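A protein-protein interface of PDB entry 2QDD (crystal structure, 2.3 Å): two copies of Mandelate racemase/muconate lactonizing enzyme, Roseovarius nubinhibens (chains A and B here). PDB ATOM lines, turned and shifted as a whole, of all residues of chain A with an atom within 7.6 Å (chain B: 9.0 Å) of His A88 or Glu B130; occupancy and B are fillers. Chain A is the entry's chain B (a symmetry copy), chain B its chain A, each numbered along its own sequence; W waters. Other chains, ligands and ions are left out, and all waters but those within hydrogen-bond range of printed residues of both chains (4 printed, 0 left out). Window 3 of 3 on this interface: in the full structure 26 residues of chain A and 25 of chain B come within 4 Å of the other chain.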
ATOM      1  N   SER A   2      23.460  11.399  25.923  1.00  0.00           N
ATOM      2  CA  SER A   2      23.809  11.247  27.365  1.00  0.00           C
ATOM      3  C   SER A   2      24.960  10.266  27.579  1.00  0.00           C
ATOM      4  O   SER A   2      25.729  10.407  28.534  1.00  0.00           O
ATOM      5  CB  SER A   2      22.586  10.814  28.180  1.00  0.00           C
ATOM      6  OG  SER A   2      22.347   9.420  28.062  1.00  0.00           O
ATOM      7  N   HIS A  77      38.437  17.385  21.175  1.00  0.00           N
ATOM      8  CA  HIS A  77      37.145  17.666  20.566  1.00  0.00           C
ATOM      9  C   HIS A  77      36.237  16.449  20.540  1.00  0.00           C
ATOM     10  O   HIS A  77      35.016  16.591  20.491  1.00  0.00           O
ATOM     11  CB  HIS A  77      37.345  18.233  19.159  1.00  0.00           C
ATOM     12  CG  HIS A  77      38.290  19.390  19.123  1.00  0.00           C
ATOM     13  ND1 HIS A  77      37.921  20.661  19.511  1.00  0.00           N
ATOM     14  CD2 HIS A  77      39.599  19.461  18.788  1.00  0.00           C
ATOM     15  CE1 HIS A  77      38.961  21.470  19.399  1.00  0.00           C
ATOM     16  NE2 HIS A  77      39.991  20.766  18.961  1.00  0.00           N
ATOM     17  N   LEU A  81      31.697  13.834  23.405  1.00  0.00           N
ATOM     18  CA  LEU A  81      30.711  13.619  22.337  1.00  0.00           C
ATOM     19  C   LEU A  81      29.931  12.327  22.547  1.00  0.00           C
ATOM     20  O   LEU A  81      30.471  11.345  23.056  1.00  0.00           O
ATOM     21  CB  LEU A  81      31.370  13.609  20.949  1.00  0.00           C
ATOM     22  CG  LEU A  81      32.010  14.888  20.401  1.00  0.00           C
ATOM     23  CD1 LEU A  81      32.576  14.647  19.005  1.00  0.00           C
ATOM     24  CD2 LEU A  81      31.051  16.072  20.384  1.00  0.00           C
ATOM     25  N   ASP A  82      28.658  12.348  22.156  1.00  0.00           N
ATOM     26  CA  ASP A  82      27.857  11.134  21.976  1.00  0.00           C
ATOM     27  C   ASP A  82      28.319  10.354  20.736  1.00  0.00           C
ATOM     28  O   ASP A  82      28.170  10.834  19.609  1.00  0.00           O
ATOM     29  CB  ASP A  82      26.368  11.506  21.863  1.00  0.00           C
ATOM     30  CG  ASP A  82      25.424  10.325  22.138  1.00  0.00           C
ATOM     31  OD1 ASP A  82      25.819   9.146  21.990  1.00  0.00           O
ATOM     32  OD2 ASP A  82      24.258  10.588  22.499  1.00  0.00           O
ATOM     33  N   ARG A  84      27.059   7.686  19.421  1.00  0.00           N
ATOM     34  CA  ARG A  84      25.957   7.132  18.633  1.00  0.00           C
ATOM     35  C   ARG A  84      25.519   8.096  17.527  1.00  0.00           C
ATOM     36  O   ARG A  84      24.882   7.679  16.559  1.00  0.00           O
ATOM     37  CB  ARG A  84      24.756   6.767  19.520  1.00  0.00           C
ATOM     38  CG  ARG A  84      25.064   5.796  20.665  1.00  0.00           C
ATOM     39  CD  ARG A  84      23.975   5.828  21.739  1.00  0.00           C
ATOM     40  NE  ARG A  84      23.844   7.133  22.392  1.00  0.00           N
ATOM     41  CZ  ARG A  84      22.949   7.426  23.338  1.00  0.00           C
ATOM     42  NH1 ARG A  84      22.090   6.508  23.767  1.00  0.00           N
ATOM     43  NH2 ARG A  84      22.913   8.645  23.858  1.00  0.00           N
ATOM     44  N   SER A  85      25.855   9.378  17.683  1.00  0.00           N
ATOM     45  CA  SER A  85      25.493  10.409  16.715  1.00  0.00           C
ATOM     46  C   SER A  85      26.561  10.552  15.626  1.00  0.00           C
ATOM     47  O   SER A  85      27.361  11.488  15.645  1.00  0.00           O
ATOM     48  CB  SER A  85      25.271  11.741  17.428  1.00  0.00           C
ATOM     49  OG  SER A  85      24.055  11.721  18.153  1.00  0.00           O
ATOM     50  N   LEU A  86      26.558   9.620  14.676  1.00  0.00           N
ATOM     51  CA  LEU A  86      27.736   9.332  13.854  1.00  0.00           C
ATOM     52  C   LEU A  86      28.059  10.403  12.821  1.00  0.00           C
ATOM     53  O   LEU A  86      29.228  10.661  12.546  1.00  0.00           O
ATOM     54  CB  LEU A  86      27.583   7.993  13.144  1.00  0.00           C
ATOM     55  CG  LEU A  86      27.701   6.734  13.997  1.00  0.00           C
ATOM     56  CD1 LEU A  86      27.443   5.561  13.106  1.00  0.00           C
ATOM     57  CD2 LEU A  86      29.083   6.632  14.579  1.00  0.00           C
ATOM     58  N   ASP A  87      27.023  11.011  12.252  1.00  0.00           N
ATOM     59  CA  ASP A  87      27.197  12.097  11.299  1.00  0.00           C
ATOM     60  C   ASP A  87      27.734  13.347  11.988  1.00  0.00           C
ATOM     61  O   ASP A  87      28.636  13.995  11.463  1.00  0.00           O
ATOM     62  CB  ASP A  87      25.885  12.390  10.560  1.00  0.00           C
ATOM     63  CG  ASP A  87      25.467  11.248   9.639  1.00  0.00           C
ATOM     64  OD1 ASP A  87      25.382  10.093  10.110  1.00  0.00           O
ATOM     65  OD2 ASP A  87      25.222  11.501   8.441  1.00  0.00           O
ATOM     66  N   HIS A  88      27.199  13.653  13.172  1.00  0.00           N
ATOM     67  CA  HIS A  88      27.701  14.751  14.000  1.00  0.00           C
ATOM     68  C   HIS A  88      29.170  14.597  14.380  1.00  0.00           C
ATOM     69  O   HIS A  88      29.930  15.558  14.291  1.00  0.00           O
ATOM     70  CB  HIS A  88      26.847  14.944  15.257  1.00  0.00           C
ATOM     71  CG  HIS A  88      27.299  16.080  16.122  1.00  0.00           C
ATOM     72  ND1 HIS A  88      27.765  15.899  17.407  1.00  0.00           N
ATOM     73  CD2 HIS A  88      27.360  17.411  15.885  1.00  0.00           C
ATOM     74  CE1 HIS A  88      28.089  17.071  17.924  1.00  0.00           C
ATOM     75  NE2 HIS A  88      27.855  18.004  17.021  1.00  0.00           N
ATOM     76  N   VAL A  89      29.565  13.388  14.775  1.00  0.00           N
ATOM     77  CA  VAL A  89      30.964  13.083  15.083  1.00  0.00           C
ATOM     78  C   VAL A  89      31.873  13.338  13.874  1.00  0.00           C
ATOM     79  O   VAL A  89      32.947  13.933  14.013  1.00  0.00           O
ATOM     80  CB  VAL A  89      31.133  11.641  15.657  1.00  0.00           C
ATOM     81  CG1 VAL A  89      32.611  11.265  15.823  1.00  0.00           C
ATOM     82  CG2 VAL A  89      30.419  11.519  17.006  1.00  0.00           C
ATOM     83  N   ASN A  90      31.418  12.923  12.691  1.00  0.00           N
ATOM     84  CA  ASN A  90      32.138  13.201  11.449  1.00  0.00           C
ATOM     85  C   ASN A  90      32.223  14.686  11.082  1.00  0.00           C
ATOM     86  O   ASN A  90      33.253  15.141  10.573  1.00  0.00           O
ATOM     87  CB  ASN A  90      31.589  12.361  10.288  1.00  0.00           C
ATOM     88  CG  ASN A  90      32.056  10.907  10.353  1.00  0.00           C
ATOM     89  OD1 ASN A  90      33.047  10.532   9.730  1.00  0.00           O
ATOM     90  ND2 ASN A  90      31.355  10.091  11.133  1.00  0.00           N
ATOM     91  N   ARG A  91      31.154  15.436  11.360  1.00  0.00           N
ATOM     92  CA  ARG A  91      31.152  16.888  11.170  1.00  0.00           C
ATOM     93  C   ARG A  91      32.148  17.639  12.051  1.00  0.00           C
ATOM     94  O   ARG A  91      32.827  18.539  11.561  1.00  0.00           O
ATOM     95  CB  ARG A  91      29.759  17.464  11.355  1.00  0.00           C
ATOM     96  CG  ARG A  91      28.834  17.167  10.200  1.00  0.00           C
ATOM     97  CD  ARG A  91      27.571  18.008  10.276  1.00  0.00           C
ATOM     98  NE  ARG A  91      26.598  17.501  11.247  1.00  0.00           N
ATOM     99  CZ  ARG A  91      25.695  16.551  11.007  1.00  0.00           C
ATOM    100  NH1 ARG A  91      25.624  15.961   9.818  1.00  0.00           N
ATOM    101  NH2 ARG A  91      24.856  16.186  11.967  1.00  0.00           N
ATOM    102  N   VAL A  92      32.240  17.256  13.328  1.00  0.00           N
ATOM    103  CA  VAL A  92      33.183  17.861  14.279  1.00  0.00           C
ATOM    104  C   VAL A  92      34.629  17.609  13.845  1.00  0.00           C
ATOM    105  O   VAL A  92      35.437  18.544  13.804  1.00  0.00           O
ATOM    106  CB  VAL A  92      32.965  17.342  15.741  1.00  0.00           C
ATOM    107  CG1 VAL A  92      34.070  17.842  16.677  1.00  0.00           C
ATOM    108  CG2 VAL A  92      31.621  17.773  16.275  1.00  0.00           C
ATOM    109  N   MET A  93      34.930  16.354  13.502  1.00  0.00           N
ATOM    110  CA  MET A  93      36.230  15.957  12.950  1.00  0.00           C
ATOM    111  C   MET A  93      36.609  16.747  11.690  1.00  0.00           C
ATOM    112  O   MET A  93      37.763  17.149  11.530  1.00  0.00           O
ATOM    113  CB  MET A  93      36.253  14.456  12.623  1.00  0.00           C
ATOM    114  CG  MET A  93      36.312  13.493  13.822  1.00  0.00           C
ATOM    115  SD  MET A  93      36.809  11.804  13.332  1.00  0.00           S
ATOM    116  CE  MET A  93      35.295  11.172  12.631  1.00  0.00           C
ATOM    117  N   ASP A  94      35.643  16.954  10.797  1.00  0.00           N
ATOM    118  CA  ASP A  94      35.883  17.728   9.577  1.00  0.00           C
ATOM    119  C   ASP A  94      36.090  19.212   9.868  1.00  0.00           C
ATOM    120  O   ASP A  94      36.855  19.881   9.177  1.00  0.00           O
ATOM    121  CB  ASP A  94      34.732  17.558   8.588  1.00  0.00           C
ATOM    122  CG  ASP A  94      34.791  16.243   7.831  1.00  0.00           C
ATOM    123  OD1 ASP A  94      35.803  15.516   7.945  1.00  0.00           O
ATOM    124  OD2 ASP A  94      33.810  15.939   7.114  1.00  0.00           O
ATOM    125  N   LEU A  95      35.388  19.709  10.885  1.00  0.00           N
ATOM    126  CA  LEU A  95      35.552  21.075  11.369  1.00  0.00           C
ATOM    127  C   LEU A  95      36.928  21.295  11.972  1.00  0.00           C
ATOM    128  O   LEU A  95      37.524  22.344  11.763  1.00  0.00           O
ATOM    129  CB  LEU A  95      34.485  21.420  12.411  1.00  0.00           C
ATOM    130  CG  LEU A  95      33.088  21.852  11.968  1.00  0.00           C
ATOM    131  CD1 LEU A  95      32.150  21.944  13.171  1.00  0.00           C
ATOM    132  CD2 LEU A  95      33.143  23.171  11.241  1.00  0.00           C
ATOM    133  N   THR A 275      31.302   5.858   7.810  1.00  0.00           N
ATOM    134  CA  THR A 275      30.190   6.767   7.524  1.00  0.00           C
ATOM    135  C   THR A 275      30.350   7.367   6.121  1.00  0.00           C
ATOM    136  O   THR A 275      29.380   7.470   5.364  1.00  0.00           O
ATOM    137  CB  THR A 275      30.062   7.877   8.603  1.00  0.00           C
ATOM    138  OG1 THR A 275      29.751   7.278   9.870  1.00  0.00           O
ATOM    139  CG2 THR A 275      28.959   8.884   8.249  1.00  0.00           C
ATOM    140  N   ARG A 276      31.585   7.727   5.776  1.00  0.00           N
ATOM    141  CA  ARG A 276      31.893   8.252   4.454  1.00  0.00           C
ATOM    142  C   ARG A 276      31.879   7.168   3.386  1.00  0.00           C
ATOM    143  O   ARG A 276      31.430   7.412   2.270  1.00  0.00           O
ATOM    144  CB  ARG A 276      33.225   9.006   4.453  1.00  0.00           C
ATOM    145  CG  ARG A 276      33.266  10.242   5.374  1.00  0.00           C
ATOM    146  CD  ARG A 276      32.480  11.423   4.822  1.00  0.00           C
ATOM    147  NE  ARG A 276      32.580  12.587   5.703  1.00  0.00           N
ATOM    148  CZ  ARG A 276      31.591  13.042   6.471  1.00  0.00           C
ATOM    149  NH1 ARG A 276      31.788  14.105   7.244  1.00  0.00           N
ATOM    150  NH2 ARG A 276      30.403  12.444   6.468  1.00  0.00           N
ATOM    151  N   PRO B 122      16.008   7.464  19.334  1.00  0.00           N
ATOM    152  CA  PRO B 122      15.116   8.268  18.513  1.00  0.00           C
ATOM    153  C   PRO B 122      15.608   8.357  17.073  1.00  0.00           C
ATOM    154  O   PRO B 122      16.811   8.257  16.826  1.00  0.00           O
ATOM    155  CB  PRO B 122      15.170   9.642  19.182  1.00  0.00           C
ATOM    156  CG  PRO B 122      16.455   9.659  19.903  1.00  0.00           C
ATOM    157  CD  PRO B 122      16.682   8.273  20.367  1.00  0.00           C
ATOM    158  N   TRP B 124      15.981  10.787  14.961  1.00  0.00           N
ATOM    159  CA  TRP B 124      16.964  11.854  14.720  1.00  0.00           C
ATOM    160  C   TRP B 124      18.406  11.478  15.057  1.00  0.00           C
ATOM    161  O   TRP B 124      19.342  12.008  14.454  1.00  0.00           O
ATOM    162  CB  TRP B 124      16.566  13.182  15.389  1.00  0.00           C
ATOM    163  CG  TRP B 124      16.416  13.113  16.884  1.00  0.00           C
ATOM    164  CD1 TRP B 124      15.248  12.988  17.581  1.00  0.00           C
ATOM    165  CD2 TRP B 124      17.463  13.172  17.865  1.00  0.00           C
ATOM    166  NE1 TRP B 124      15.500  12.964  18.929  1.00  0.00           N
ATOM    167  CE2 TRP B 124      16.851  13.068  19.132  1.00  0.00           C
ATOM    168  CE3 TRP B 124      18.856  13.293  17.798  1.00  0.00           C
ATOM    169  CZ2 TRP B 124      17.585  13.081  20.323  1.00  0.00           C
ATOM    170  CZ3 TRP B 124      19.584  13.295  18.983  1.00  0.00           C
ATOM    171  CH2 TRP B 124      18.944  13.200  20.229  1.00  0.00           C
ATOM    172  N   GLN B 125      18.577  10.564  16.012  1.00  0.00           N
ATOM    173  CA  GLN B 125      19.899  10.051  16.370  1.00  0.00           C
ATOM    174  C   GLN B 125      20.393   8.970  15.415  1.00  0.00           C
ATOM    175  O   GLN B 125      21.585   8.917  15.087  1.00  0.00           O
ATOM    176  CB  GLN B 125      19.914   9.537  17.807  1.00  0.00           C
ATOM    177  CG  GLN B 125      21.304   9.201  18.318  1.00  0.00           C
ATOM    178  CD  GLN B 125      21.472   9.469  19.799  1.00  0.00           C
ATOM    179  OE1 GLN B 125      22.404  10.158  20.214  1.00  0.00           O
ATOM    180  NE2 GLN B 125      20.572   8.922  20.605  1.00  0.00           N
ATOM    181  N   LEU B 126      19.480   8.111  14.968  1.00  0.00           N
ATOM    182  CA  LEU B 126      19.801   7.111  13.943  1.00  0.00           C
ATOM    183  C   LEU B 126      20.163   7.770  12.617  1.00  0.00           C
ATOM    184  O   LEU B 126      20.964   7.235  11.850  1.00  0.00           O
ATOM    185  CB  LEU B 126      18.638   6.138  13.745  1.00  0.00           C
ATOM    186  CG  LEU B 126      18.446   5.023  14.775  1.00  0.00           C
ATOM    187  CD1 LEU B 126      17.171   4.269  14.462  1.00  0.00           C
ATOM    188  CD2 LEU B 126      19.632   4.075  14.791  1.00  0.00           C
ATOM    189  N   LEU B 127      19.578   8.941  12.377  1.00  0.00           N
ATOM    190  CA  LEU B 127      19.888   9.755  11.211  1.00  0.00           C
ATOM    191  C   LEU B 127      21.108  10.658  11.407  1.00  0.00           C
ATOM    192  O   LEU B 127      21.521  11.358  10.488  1.00  0.00           O
ATOM    193  CB  LEU B 127      18.653  10.558  10.787  1.00  0.00           C
ATOM    194  CG  LEU B 127      17.504   9.670  10.298  1.00  0.00           C
ATOM    195  CD1 LEU B 127      16.162  10.376  10.384  1.00  0.00           C
ATOM    196  CD2 LEU B 127      17.766   9.137   8.895  1.00  0.00           C
ATOM    197  N   GLY B 128      21.679  10.634  12.607  1.00  0.00           N
ATOM    198  CA  GLY B 128      23.035  11.121  12.836  1.00  0.00           C
ATOM    199  C   GLY B 128      23.117  12.444  13.571  1.00  0.00           C
ATOM    200  O   GLY B 128      24.209  12.972  13.764  1.00  0.00           O
ATOM    201  N   GLY B 129      21.969  12.982  13.984  1.00  0.00           N
ATOM    202  CA  GLY B 129      21.915  14.289  14.646  1.00  0.00           C
ATOM    203  C   GLY B 129      22.411  14.257  16.083  1.00  0.00           C
ATOM    204  O   GLY B 129      22.307  13.228  16.753  1.00  0.00           O
ATOM    205  N   GLU B 130      22.946  15.382  16.553  1.00  0.00           N
ATOM    206  CA  GLU B 130      23.450  15.493  17.928  1.00  0.00           C
ATOM    207  C   GLU B 130      22.361  15.692  18.975  1.00  0.00           C
ATOM    208  O   GLU B 130      22.541  15.334  20.138  1.00  0.00           O
ATOM    209  CB  GLU B 130      24.491  16.615  18.057  1.00  0.00           C
ATOM    210  CG  GLU B 130      24.024  18.015  17.656  1.00  0.00           C
ATOM    211  CD  GLU B 130      24.859  19.125  18.288  1.00  0.00           C
ATOM    212  OE1 GLU B 130      24.879  20.240  17.722  1.00  0.00           O
ATOM    213  OE2 GLU B 130      25.491  18.890  19.346  1.00  0.00           O
ATOM    214  N   ALA B 131      21.245  16.283  18.557  1.00  0.00           N
ATOM    215  CA  ALA B 131      20.239  16.790  19.476  1.00  0.00           C
ATOM    216  C   ALA B 131      18.877  16.780  18.796  1.00  0.00           C
ATOM    217  O   ALA B 131      18.793  16.793  17.568  1.00  0.00           O
ATOM    218  CB  ALA B 131      20.597  18.202  19.931  1.00  0.00           C
ATOM    219  N   ALA B 132      17.816  16.769  19.601  1.00  0.00           N
ATOM    220  CA  ALA B 132      16.471  17.083  19.130  1.00  0.00           C
ATOM    221  C   ALA B 132      16.339  18.579  18.859  1.00  0.00           C
ATOM    222  O   ALA B 132      15.726  19.317  19.641  1.00  0.00           O
ATOM    223  CB  ALA B 132      15.429  16.614  20.143  1.00  0.00           C
ATOM    224  N   THR B 133      16.928  19.017  17.748  1.00  0.00           N
ATOM    225  CA  THR B 133      17.007  20.430  17.390  1.00  0.00           C
ATOM    226  C   THR B 133      15.610  20.948  17.052  1.00  0.00           C
ATOM    227  O   THR B 133      14.906  20.335  16.249  1.00  0.00           O
ATOM    228  CB  THR B 133      17.977  20.646  16.200  1.00  0.00           C
ATOM    229  OG1 THR B 133      19.285  20.190  16.565  1.00  0.00           O
ATOM    230  CG2 THR B 133      18.066  22.114  15.812  1.00  0.00           C
ATOM    231  N   ARG B 281      19.302  13.862   1.322  1.00  0.00           N
ATOM    232  CA  ARG B 281      19.735  14.844   2.318  1.00  0.00           C
ATOM    233  C   ARG B 281      21.254  14.942   2.388  1.00  0.00           C
ATOM    234  O   ARG B 281      21.813  16.041   2.361  1.00  0.00           O
ATOM    235  CB  ARG B 281      19.174  14.490   3.702  1.00  0.00           C
ATOM    236  CG  ARG B 281      19.276  15.622   4.733  1.00  0.00           C
ATOM    237  CD  ARG B 281      20.565  15.567   5.555  1.00  0.00           C
ATOM    238  NE  ARG B 281      20.804  14.270   6.206  1.00  0.00           N
ATOM    239  CZ  ARG B 281      20.322  13.925   7.397  1.00  0.00           C
ATOM    240  NH1 ARG B 281      19.545  14.762   8.071  1.00  0.00           N
ATOM    241  NH2 ARG B 281      20.613  12.736   7.917  1.00  0.00           N
ATOM    242  N   HIS B 308      12.207  14.536  12.175  1.00  0.00           N
ATOM    243  CA  HIS B 308      13.396  13.790  12.588  1.00  0.00           C
ATOM    244  C   HIS B 308      14.559  13.953  11.600  1.00  0.00           C
ATOM    245  O   HIS B 308      15.716  14.078  12.016  1.00  0.00           O
ATOM    246  CB  HIS B 308      13.067  12.299  12.750  1.00  0.00           C
ATOM    247  CG  HIS B 308      12.449  11.946  14.069  1.00  0.00           C
ATOM    248  ND1 HIS B 308      13.151  11.975  15.254  1.00  0.00           N
ATOM    249  CD2 HIS B 308      11.201  11.524  14.385  1.00  0.00           C
ATOM    250  CE1 HIS B 308      12.359  11.602  16.243  1.00  0.00           C
ATOM    251  NE2 HIS B 308      11.171  11.323  15.742  1.00  0.00           N
ATOM    252  N   ALA B 311      15.692  17.797  11.777  1.00  0.00           N
ATOM    253  CA  ALA B 311      16.476  18.122  12.977  1.00  0.00           C
ATOM    254  C   ALA B 311      17.899  17.589  12.919  1.00  0.00           C
ATOM    255  O   ALA B 311      18.821  18.216  13.436  1.00  0.00           O
ATOM    256  CB  ALA B 311      15.778  17.609  14.222  1.00  0.00           C
ATOM    257  N   SER B 312      18.072  16.435  12.279  1.00  0.00           N
ATOM    258  CA  SER B 312      19.387  15.806  12.123  1.00  0.00           C
ATOM    259  C   SER B 312      20.223  16.429  10.996  1.00  0.00           C
ATOM    260  O   SER B 312      21.382  16.059  10.799  1.00  0.00           O
ATOM    261  CB  SER B 312      19.210  14.307  11.878  1.00  0.00           C
ATOM    262  OG  SER B 312      18.470  14.082  10.691  1.00  0.00           O
ATOM    263  N   THR B 313      19.628  17.362  10.256  1.00  0.00           N
ATOM    264  CA  THR B 313      20.284  18.048   9.140  1.00  0.00           C
ATOM    265  C   THR B 313      21.060  19.248   9.685  1.00  0.00           C
ATOM    266  O   THR B 313      20.501  20.029  10.457  1.00  0.00           O
ATOM    267  CB  THR B 313      19.214  18.512   8.119  1.00  0.00           C
ATOM    268  OG1 THR B 313      18.560  17.363   7.567  1.00  0.00           O
ATOM    269  CG2 THR B 313      19.798  19.368   7.000  1.00  0.00           C
ATOM    270  N   PRO B 314      22.351  19.389   9.298  1.00  0.00           N
ATOM    271  CA  PRO B 314      23.204  20.530   9.688  1.00  0.00           C
ATOM    272  C   PRO B 314      22.534  21.895   9.513  1.00  0.00           C
ATOM    273  O   PRO B 314      21.816  22.113   8.531  1.00  0.00           O
ATOM    274  CB  PRO B 314      24.402  20.415   8.743  1.00  0.00           C
ATOM    275  CG  PRO B 314      24.477  18.969   8.397  1.00  0.00           C
ATOM    276  CD  PRO B 314      23.084  18.415   8.461  1.00  0.00           C
ATOM    277  N   GLU B 315      22.774  22.791  10.468  1.00  0.00           N
ATOM    278  CA  GLU B 315      22.100  24.095  10.542  1.00  0.00           C
ATOM    279  C   GLU B 315      22.222  24.932   9.255  1.00  0.00           C
ATOM    280  O   GLU B 315      21.257  25.573   8.833  1.00  0.00           O
ATOM    281  CB  GLU B 315      22.584  24.870  11.787  1.00  0.00           C
ATOM    282  CG  GLU B 315      22.387  26.399  11.776  1.00  0.00           C
ATOM    283  CD  GLU B 315      20.993  26.836  12.215  1.00  0.00           C
ATOM    284  OE1 GLU B 315      20.882  27.474  13.286  1.00  0.00           O
ATOM    285  OE2 GLU B 315      20.011  26.556  11.488  1.00  0.00           O
ATOM    286  N   ARG B 318      19.807  23.420   6.596  1.00  0.00           N
ATOM    287  CA  ARG B 318      18.415  23.226   6.967  1.00  0.00           C
ATOM    288  C   ARG B 318      17.669  24.550   6.897  1.00  0.00           C
ATOM    289  O   ARG B 318      18.119  25.555   7.444  1.00  0.00           O
ATOM    290  CB  ARG B 318      18.317  22.609   8.362  1.00  0.00           C
ATOM    291  CG  ARG B 318      16.901  22.248   8.813  1.00  0.00           C
ATOM    292  CD  ARG B 318      16.739  22.501  10.304  1.00  0.00           C
ATOM    293  NE  ARG B 318      17.731  21.752  11.073  1.00  0.00           N
ATOM    294  CZ  ARG B 318      18.525  22.270  12.004  1.00  0.00           C
ATOM    295  NH1 ARG B 318      19.396  21.490  12.631  1.00  0.00           N
ATOM    296  NH2 ARG B 318      18.450  23.560  12.318  1.00  0.00           N
ATOM    297  N   SER B 349      12.195  12.455  21.629  1.00  0.00           N
ATOM    298  CA  SER B 349      13.451  11.757  21.915  1.00  0.00           C
ATOM    299  C   SER B 349      13.258  10.320  22.406  1.00  0.00           C
ATOM    300  O   SER B 349      14.231   9.617  22.689  1.00  0.00           O
ATOM    301  CB  SER B 349      14.283  12.560  22.906  1.00  0.00           C
ATOM    302  OG  SER B 349      14.687  13.787  22.326  1.00  0.00           O
HETATM  303  O   HOH W   1      23.847   7.376  13.944  1.00  0.00           O
HETATM  304  O   HOH W   2      22.759  10.754   7.424  1.00  0.00           O
HETATM  305  O   HOH W   3      23.570  17.616  13.934  1.00  0.00           O
HETATM  306  O   HOH W   4      23.041  14.272  10.356  1.00  0.00           O
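The side-chain carboxylate (OD2) of Asp A82 lies close to the side-chain amide oxygen (OE1) of Gln B125 (3.0 Å). OE1 of Gln B125 lies within hydrogen-bond range of OG of Ser A85, at 3.1 Å. The backbone carbonyl oxygen (O) of Gly B128 sits at hydrogen-bond distance from the backbone NH (N) of His A88 (3.1 Å). OG of Ser A85 is in hydrogen-bond range of O of Gly B129 (2.7 Å). The side-chain carboxylate (OE2) of Glu B130 sits at hydrogen-bond distance from a ring nitrogen (NE2) of His A88, 3.4 Å away.
O of Trp B124 lies within hydrogen-bond range of N of Gly B129, at 2.8 Å. The guanidinium group of Arg B281 is in hydrogen-bond range of the side-chain hydroxyl of Ser B312, at 2.9 Å. OG of Ser B312 sits at hydrogen-bond distance from O of His B308, at 3.1 Å. The side-chain carboxylate (OD2) of Asp A82 lies within salt-bridge range of the guanidinium group (NH2) of Arg A84.
Gln B125 touches Arg A84 (O to O, 3.8 Å). Gly B128 touches Ser A85 (O to C, 3.9 Å). Ser A85 touches Glu B130. Gly B128 touches Asp A87. Arg A91 touches Gly B128 (NH2 to O, 3.7 Å). Arg A91 touches Ser B312. CG of Pro B314 touches NH1 of Arg A91, 3.5 Å away.
His A88 touches two residues of chain B. Of the printed residues of chain A, Gly B129 touches Ser A85 (2.7 Å). Of the printed residues of chain A, Ser B312 touches Arg A91 (3.7 Å). Printed residues of chain A within 4 Å of Gly B128: Ser A85, Asp A87, His A88 and Arg A91. The nearest printed residue of chain A that does not touch Gly B129 is Arg A91 (4.4 Å).
Of the 20 printed residues of chain B, 6 touch a printed residue of chain A. Hydrophobic or aromatic side chains of chain B within 4 Å of the printed part of chain A: Pro B314. Along chain B the printed residues that touch a printed residue of chain A span positions 125 to 314. Of the 18 printed residues of chain A, 6 touch a printed residue of chain B. Hydrophobic or aromatic side chains of chain A that line the printed part of chain B: His A88. Among the printed residues, 12 pairs touch across the chains.
No position is printed for both chains. Of the 12 pairs that touch across the chains among the printed residues, none has its exchanged pair printed and touching as well.
Water W4 lies within hydrogen-bond range of O of Ser B312, NH2 of Arg A91 and O of Leu B127. Water W3 lies within hydrogen-bond range of the guanidinium group of Arg A91 (2.8 Å) and the backbone NH of Glu B130 (3.5 Å). Water W2 lies within hydrogen-bond range of the side-chain carboxylate (OD2) of Asp A87 (2.8 Å), the guanidinium group (NH2) of Arg B281 (3.0 Å) and the backbone carbonyl oxygen (O) of Leu B127 (3.4 Å). Water W1 lies within hydrogen-bond range of O of Arg A84 (2.8 Å) and O of Gln B125 (3.0 Å).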
